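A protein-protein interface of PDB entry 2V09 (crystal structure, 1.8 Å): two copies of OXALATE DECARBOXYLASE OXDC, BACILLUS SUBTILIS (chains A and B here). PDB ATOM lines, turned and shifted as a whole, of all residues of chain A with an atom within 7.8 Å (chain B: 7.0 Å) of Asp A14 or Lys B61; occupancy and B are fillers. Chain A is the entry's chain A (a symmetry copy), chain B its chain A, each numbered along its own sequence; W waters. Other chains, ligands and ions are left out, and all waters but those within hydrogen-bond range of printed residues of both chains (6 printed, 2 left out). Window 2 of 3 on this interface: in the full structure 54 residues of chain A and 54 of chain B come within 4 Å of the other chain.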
ATOM      1  N   ILE A  11      23.322 -17.336   5.961  1.00  0.00           N
ATOM      2  CA  ILE A  11      22.437 -18.257   5.240  1.00  0.00           C
ATOM      3  C   ILE A  11      21.929 -17.554   3.965  1.00  0.00           C
ATOM      4  O   ILE A  11      21.452 -16.418   4.026  1.00  0.00           O
ATOM      5  CB  ILE A  11      21.248 -18.749   6.132  1.00  0.00           C
ATOM      6  CG1 ILE A  11      21.751 -19.531   7.362  1.00  0.00           C
ATOM      7  CG2 ILE A  11      20.222 -19.569   5.239  1.00  0.00           C
ATOM      8  CD1 ILE A  11      20.733 -19.746   8.503  1.00  0.00           C
ATOM      9  N   ARG A  12      22.015 -18.238   2.823  1.00  0.00           N
ATOM     10  CA  ARG A  12      21.534 -17.737   1.538  1.00  0.00           C
ATOM     11  C   ARG A  12      20.863 -18.952   0.896  1.00  0.00           C
ATOM     12  O   ARG A  12      21.513 -19.896   0.412  1.00  0.00           O
ATOM     13  CB  ARG A  12      22.678 -17.154   0.694  1.00  0.00           C
ATOM     14  CG  ARG A  12      22.360 -16.587  -0.710  1.00  0.00           C
ATOM     15  CD  ARG A  12      23.670 -16.042  -1.358  1.00  0.00           C
ATOM     16  NE  ARG A  12      24.475 -17.149  -1.797  1.00  0.00           N
ATOM     17  CZ  ARG A  12      25.742 -17.369  -1.541  1.00  0.00           C
ATOM     18  NH1 ARG A  12      26.529 -16.513  -0.856  1.00  0.00           N
ATOM     19  NH2 ARG A  12      26.250 -18.487  -2.003  1.00  0.00           N
ATOM     20  N   GLY A  13      19.543 -18.965   0.993  1.00  0.00           N
ATOM     21  CA  GLY A  13      18.757 -20.121   0.485  1.00  0.00           C
ATOM     22  C   GLY A  13      19.101 -21.392   1.253  1.00  0.00           C
ATOM     23  O   GLY A  13      19.061 -21.414   2.483  1.00  0.00           O
ATOM     24  N   ASP A  14      19.528 -22.402   0.515  1.00  0.00           N
ATOM     25  CA  ASP A  14      19.930 -23.677   1.081  1.00  0.00           C
ATOM     26  C   ASP A  14      21.451 -23.754   1.409  1.00  0.00           C
ATOM     27  O   ASP A  14      21.966 -24.798   1.794  1.00  0.00           O
ATOM     28  CB  ASP A  14      19.465 -24.815   0.161  1.00  0.00           C
ATOM     29  CG  ASP A  14      19.999 -24.722  -1.273  1.00  0.00           C
ATOM     30  OD1 ASP A  14      20.886 -23.864  -1.601  1.00  0.00           O
ATOM     31  OD2 ASP A  14      19.527 -25.530  -2.130  1.00  0.00           O
ATOM     32  N   LYS A  15      22.160 -22.638   1.275  1.00  0.00           N
ATOM     33  CA  LYS A  15      23.573 -22.554   1.636  1.00  0.00           C
ATOM     34  C   LYS A  15      23.811 -21.829   2.951  1.00  0.00           C
ATOM     35  O   LYS A  15      23.062 -20.917   3.327  1.00  0.00           O
ATOM     36  CB  LYS A  15      24.347 -21.849   0.542  1.00  0.00           C
ATOM     37  CG  LYS A  15      24.386 -22.679  -0.760  1.00  0.00           C
ATOM     38  CD  LYS A  15      25.110 -21.984  -1.911  1.00  0.00           C
ATOM     39  CE  LYS A  15      25.065 -22.885  -3.151  1.00  0.00           C
ATOM     40  NZ  LYS A  15      25.855 -22.343  -4.331  1.00  0.00           N
ATOM     41  N   GLY A  16      24.930 -22.169   3.581  1.00  0.00           N
ATOM     42  CA  GLY A  16      25.296 -21.603   4.877  1.00  0.00           C
ATOM     43  C   GLY A  16      24.558 -22.242   6.039  1.00  0.00           C
ATOM     44  O   GLY A  16      23.900 -23.285   5.902  1.00  0.00           O
ATOM     45  N   ALA A  17      24.666 -21.592   7.196  1.00  0.00           N
ATOM     46  CA  ALA A  17      24.182 -22.118   8.437  1.00  0.00           C
ATOM     47  C   ALA A  17      24.243 -20.996   9.495  1.00  0.00           C
ATOM     48  O   ALA A  17      24.865 -19.952   9.302  1.00  0.00           O
ATOM     49  CB  ALA A  17      25.008 -23.381   8.890  1.00  0.00           C
ATOM     50  N   LEU B  59      29.695 -19.561   1.632  1.00  0.00           N
ATOM     51  CA  LEU B  59      28.540 -20.380   2.000  1.00  0.00           C
ATOM     52  C   LEU B  59      28.373 -21.539   1.023  1.00  0.00           C
ATOM     53  O   LEU B  59      28.409 -21.333  -0.222  1.00  0.00           O
ATOM     54  CB  LEU B  59      27.286 -19.515   1.996  1.00  0.00           C
ATOM     55  CG  LEU B  59      27.318 -18.160   2.745  1.00  0.00           C
ATOM     56  CD1 LEU B  59      25.932 -17.484   2.737  1.00  0.00           C
ATOM     57  CD2 LEU B  59      27.856 -18.330   4.169  1.00  0.00           C
ATOM     58  N   GLU B  60      28.166 -22.729   1.591  1.00  0.00           N
ATOM     59  CA  GLU B  60      27.931 -23.937   0.808  1.00  0.00           C
ATOM     60  C   GLU B  60      26.716 -24.690   1.360  1.00  0.00           C
ATOM     61  O   GLU B  60      26.245 -24.408   2.446  1.00  0.00           O
ATOM     62  CB  GLU B  60      29.173 -24.848   0.831  1.00  0.00           C
ATOM     63  CG  GLU B  60      30.455 -24.235   0.173  1.00  0.00           C
ATOM     64  CD  GLU B  60      30.351 -23.987  -1.333  1.00  0.00           C
ATOM     65  OE1 GLU B  60      29.407 -24.507  -2.000  1.00  0.00           O
ATOM     66  OE2 GLU B  60      31.211 -23.233  -1.868  1.00  0.00           O
ATOM     67  N   LYS B  61      26.216 -25.646   0.576  1.00  0.00           N
ATOM     68  CA  LYS B  61      25.170 -26.565   1.048  1.00  0.00           C
ATOM     69  C   LYS B  61      25.872 -27.480   2.042  1.00  0.00           C
ATOM     70  O   LYS B  61      26.689 -28.297   1.668  1.00  0.00           O
ATOM     71  CB  LYS B  61      24.524 -27.357  -0.093  1.00  0.00           C
ATOM     72  CG  LYS B  61      23.833 -26.506  -1.104  1.00  0.00           C
ATOM     73  CD  LYS B  61      23.104 -27.399  -2.099  1.00  0.00           C
ATOM     74  CE  LYS B  61      22.666 -26.609  -3.286  1.00  0.00           C
ATOM     75  NZ  LYS B  61      21.537 -27.380  -3.994  1.00  0.00           N
ATOM     76  N   GLY B  62      25.614 -27.217   3.320  1.00  0.00           N
ATOM     77  CA  GLY B  62      26.205 -27.944   4.420  1.00  0.00           C
ATOM     78  C   GLY B  62      27.037 -27.112   5.388  1.00  0.00           C
ATOM     79  O   GLY B  62      27.521 -27.648   6.374  1.00  0.00           O
ATOM     80  N   GLY B  63      27.239 -25.819   5.092  1.00  0.00           N
ATOM     81  CA  GLY B  63      28.009 -24.969   6.002  1.00  0.00           C
ATOM     82  C   GLY B  63      28.623 -23.736   5.396  1.00  0.00           C
ATOM     83  O   GLY B  63      28.133 -23.185   4.415  1.00  0.00           O
ATOM     84  N   TYR B  64      29.699 -23.296   6.046  1.00  0.00           N
ATOM     85  CA  TYR B  64      30.434 -22.125   5.598  1.00  0.00           C
ATOM     86  C   TYR B  64      31.904 -22.181   6.066  1.00  0.00           C
ATOM     87  O   TYR B  64      32.304 -22.960   6.974  1.00  0.00           O
ATOM     88  CB  TYR B  64      29.748 -20.811   6.041  1.00  0.00           C
ATOM     89  CG  TYR B  64      29.684 -20.550   7.570  1.00  0.00           C
ATOM     90  CD1 TYR B  64      30.814 -20.182   8.307  1.00  0.00           C
ATOM     91  CD2 TYR B  64      28.462 -20.620   8.258  1.00  0.00           C
ATOM     92  CE1 TYR B  64      30.724 -19.917   9.671  1.00  0.00           C
ATOM     93  CE2 TYR B  64      28.372 -20.355   9.630  1.00  0.00           C
ATOM     94  CZ  TYR B  64      29.478 -20.043  10.323  1.00  0.00           C
ATOM     95  OH  TYR B  64      29.363 -19.813  11.651  1.00  0.00           O
ATOM     96  N   LYS B  87      27.049 -28.321   9.060  1.00  0.00           N
ATOM     97  CA  LYS B  87      25.750 -28.823   9.524  1.00  0.00           C
ATOM     98  C   LYS B  87      25.820 -30.313   9.844  1.00  0.00           C
ATOM     99  O   LYS B  87      26.780 -30.994   9.453  1.00  0.00           O
ATOM    100  CB  LYS B  87      24.687 -28.536   8.442  1.00  0.00           C
ATOM    101  CG  LYS B  87      24.403 -27.038   8.241  1.00  0.00           C
ATOM    102  CD  LYS B  87      23.618 -26.805   6.987  1.00  0.00           C
ATOM    103  CE  LYS B  87      22.154 -27.185   7.114  1.00  0.00           C
ATOM    104  NZ  LYS B  87      21.448 -27.123   5.797  1.00  0.00           N
ATOM    105  N   ALA B  90      27.185 -33.084   7.435  1.00  0.00           N
ATOM    106  CA  ALA B  90      27.864 -32.424   6.326  1.00  0.00           C
ATOM    107  C   ALA B  90      29.341 -32.763   6.331  1.00  0.00           C
ATOM    108  O   ALA B  90      29.957 -32.970   7.393  1.00  0.00           O
ATOM    109  CB  ALA B  90      27.632 -30.916   6.293  1.00  0.00           C
ATOM    110  N   ILE B  91      29.876 -32.846   5.113  1.00  0.00           N
ATOM    111  CA  ILE B  91      31.218 -33.351   4.860  1.00  0.00           C
ATOM    112  C   ILE B  91      32.097 -32.272   4.254  1.00  0.00           C
ATOM    113  O   ILE B  91      31.730 -31.652   3.284  1.00  0.00           O
ATOM    114  CB  ILE B  91      31.201 -34.585   3.931  1.00  0.00           C
ATOM    115  CG1 ILE B  91      30.545 -35.796   4.602  1.00  0.00           C
ATOM    116  CG2 ILE B  91      32.676 -34.905   3.418  1.00  0.00           C
ATOM    117  CD1 ILE B  91      30.215 -36.910   3.601  1.00  0.00           C
ATOM    118  N   LYS B 199      33.190 -30.789  -4.830  1.00  0.00           N
ATOM    119  CA  LYS B 199      32.081 -30.683  -3.866  1.00  0.00           C
ATOM    120  C   LYS B 199      32.412 -29.651  -2.770  1.00  0.00           C
ATOM    121  O   LYS B 199      31.606 -28.802  -2.486  1.00  0.00           O
ATOM    122  CB  LYS B 199      31.756 -32.068  -3.283  1.00  0.00           C
ATOM    123  CG  LYS B 199      31.235 -33.066  -4.327  1.00  0.00           C
ATOM    124  CD  LYS B 199      30.589 -34.327  -3.727  1.00  0.00           C
ATOM    125  CE  LYS B 199      29.952 -35.210  -4.780  1.00  0.00           C
ATOM    126  NZ  LYS B 199      29.088 -36.284  -4.129  1.00  0.00           N
ATOM    127  N   ILE B 201      32.277 -28.645   0.360  1.00  0.00           N
ATOM    128  CA  ILE B 201      31.410 -28.924   1.520  1.00  0.00           C
ATOM    129  C   ILE B 201      30.106 -29.414   0.938  1.00  0.00           C
ATOM    130  O   ILE B 201      29.565 -28.801   0.024  1.00  0.00           O
ATOM    131  CB  ILE B 201      31.167 -27.705   2.449  1.00  0.00           C
ATOM    132  CG1 ILE B 201      32.464 -27.336   3.214  1.00  0.00           C
ATOM    133  CG2 ILE B 201      30.003 -27.950   3.424  1.00  0.00           C
ATOM    134  CD1 ILE B 201      32.347 -26.064   3.985  1.00  0.00           C
ATOM    135  N   PHE B 202      29.596 -30.536   1.440  1.00  0.00           N
ATOM    136  CA  PHE B 202      28.341 -31.076   0.930  1.00  0.00           C
ATOM    137  C   PHE B 202      27.521 -31.764   2.026  1.00  0.00           C
ATOM    138  O   PHE B 202      28.084 -32.343   2.964  1.00  0.00           O
ATOM    139  CB  PHE B 202      28.545 -31.971  -0.304  1.00  0.00           C
ATOM    140  CG  PHE B 202      29.424 -33.185  -0.101  1.00  0.00           C
ATOM    141  CD1 PHE B 202      30.819 -33.076  -0.043  1.00  0.00           C
ATOM    142  CD2 PHE B 202      28.855 -34.454  -0.054  1.00  0.00           C
ATOM    143  CE1 PHE B 202      31.623 -34.252   0.103  1.00  0.00           C
ATOM    144  CE2 PHE B 202      29.624 -35.603   0.041  1.00  0.00           C
ATOM    145  CZ  PHE B 202      31.017 -35.500   0.157  1.00  0.00           C
ATOM    146  N   GLU B 203      26.201 -31.701   1.866  1.00  0.00           N
ATOM    147  CA  GLU B 203      25.271 -32.323   2.827  1.00  0.00           C
ATOM    148  C   GLU B 203      25.362 -33.836   2.682  1.00  0.00           C
ATOM    149  O   GLU B 203      25.554 -34.364   1.574  1.00  0.00           O
ATOM    150  CB  GLU B 203      23.823 -31.881   2.569  1.00  0.00           C
ATOM    151  CG  GLU B 203      23.536 -30.391   2.539  1.00  0.00           C
ATOM    152  CD  GLU B 203      23.198 -29.749   3.901  1.00  0.00           C
ATOM    153  OE1 GLU B 203      23.609 -30.256   4.988  1.00  0.00           O
ATOM    154  OE2 GLU B 203      22.569 -28.667   3.897  1.00  0.00           O
ATOM    155  N   ASN B 204      25.163 -34.566   3.771  1.00  0.00           N
ATOM    156  CA  ASN B 204      25.133 -36.013   3.736  1.00  0.00           C
ATOM    157  C   ASN B 204      24.395 -36.578   4.980  1.00  0.00           C
ATOM    158  O   ASN B 204      24.298 -35.915   6.026  1.00  0.00           O
ATOM    159  CB  ASN B 204      26.566 -36.548   3.602  1.00  0.00           C
ATOM    160  CG  ASN B 204      26.714 -37.525   2.427  1.00  0.00           C
ATOM    161  OD1 ASN B 204      26.944 -38.638   2.664  1.00  0.00           O
ATOM    162  ND2 ASN B 204      26.507 -37.082   1.175  1.00  0.00           N
HETATM  163  O   HOH W   1      28.922 -19.603  -2.217  1.00  0.00           O
HETATM  164  O   HOH W   2      19.617 -25.386  -4.874  1.00  0.00           O
HETATM  165  O   HOH W   3      19.358 -28.550  -2.095  1.00  0.00           O
HETATM  166  O   HOH W   4      29.365 -17.081  -0.026  1.00  0.00           O
HETATM  167  O   HOH W   5      21.464 -27.576   1.914  1.00  0.00           O
HETATM  168  O   HOH W   6      28.464 -21.960  -3.371  1.00  0.00           O
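Of the 7 printed residues of chain A, 5 touch a printed residue of chain B.
Hydrophobic or aromatic side chains of chain A within 4 Å of the printed part of chain B: Ala A17.
Among the printed residues, 11 pairs touch across the chains.
Among the printed residues, Asp or Glu carboxylates within 4 Å of a Lys or Arg side-chain nitrogen of the other chain: Asp A14 with Lys B61.
The backbone NH (N) of Gly A16 lies within hydrogen-bond range of the backbone carbonyl oxygen (O) of Glu B60 (2.8 Å).
NZ of Lys B61 is in salt-bridge range of OD2 of Asp A14.
The backbone carbonyl oxygen of Gly B63 lies close to the backbone NH of Gly A16 (3.5 Å).
O of Gly B62 sits at hydrogen-bond distance from N of Lys B87 (2.8 Å).
The side-chain amino group (NZ) of Lys B87 is in salt-bridge range of the side-chain carboxylate (OE2) of Glu B203 (2.7 Å).
The backbone carbonyl oxygen of Lys B61 is in hydrogen-bond range of the backbone NH of Glu B203.
Water W5 lies within hydrogen-bond range of the side-chain carboxylate of Glu B203 and the backbone carbonyl oxygen of Asp A14.
Water W1 bridges O of Leu B59 (2.7 Å) and NH2 of Arg A12 (2.9 Å).
Water W2 bridges OD2 of Asp A14 (2.7 Å) and NZ of Lys B61 (2.9 Å).
Water W6 lies within hydrogen-bond range of NZ of Lys A15, OE1 of Glu B60 and O of Leu B59.
Water W4 bridges the backbone NH of Leu B59 (3.0 Å) and the guanidinium group of Arg A12 (3.0 Å).
Water W3 lies within hydrogen-bond range of the side-chain carboxylate (OD2) of Asp A14 and the side-chain amino group (NZ) of Lys B61.
Printed residues of chain B within 4 Å of Arg A12: Leu B59.
Of the printed residues of chain B, Asp A14 touches Lys B61 (3.3 Å).
Of the printed residues of chain B, Lys A15 touches Leu B59 (3.8 Å), Glu B60 (3.4 Å) and Lys B61 (3.7 Å).
The nearest residue of chain A that does not touch Lys B61 is Gly A16 (4.8 Å).
Arg A12 touches Leu B59.
Leu B59 touches Lys A15 (O to CD, 3.8 Å).
Lys A15 touches Glu B60.
Lys A15 touches Lys B61 (CG to N, 3.7 Å).
Gly A16 touches Leu B59.
Lys B87 touches Gly A16.
Ala A17 touches Tyr B64.
CG of Lys B87 touches CB of Ala A17 (3.8 Å).
No position is printed for both chains.
Of the 11 pairs that touch across the chains among the printed residues, none has its exchanged pair printed and touching as well.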
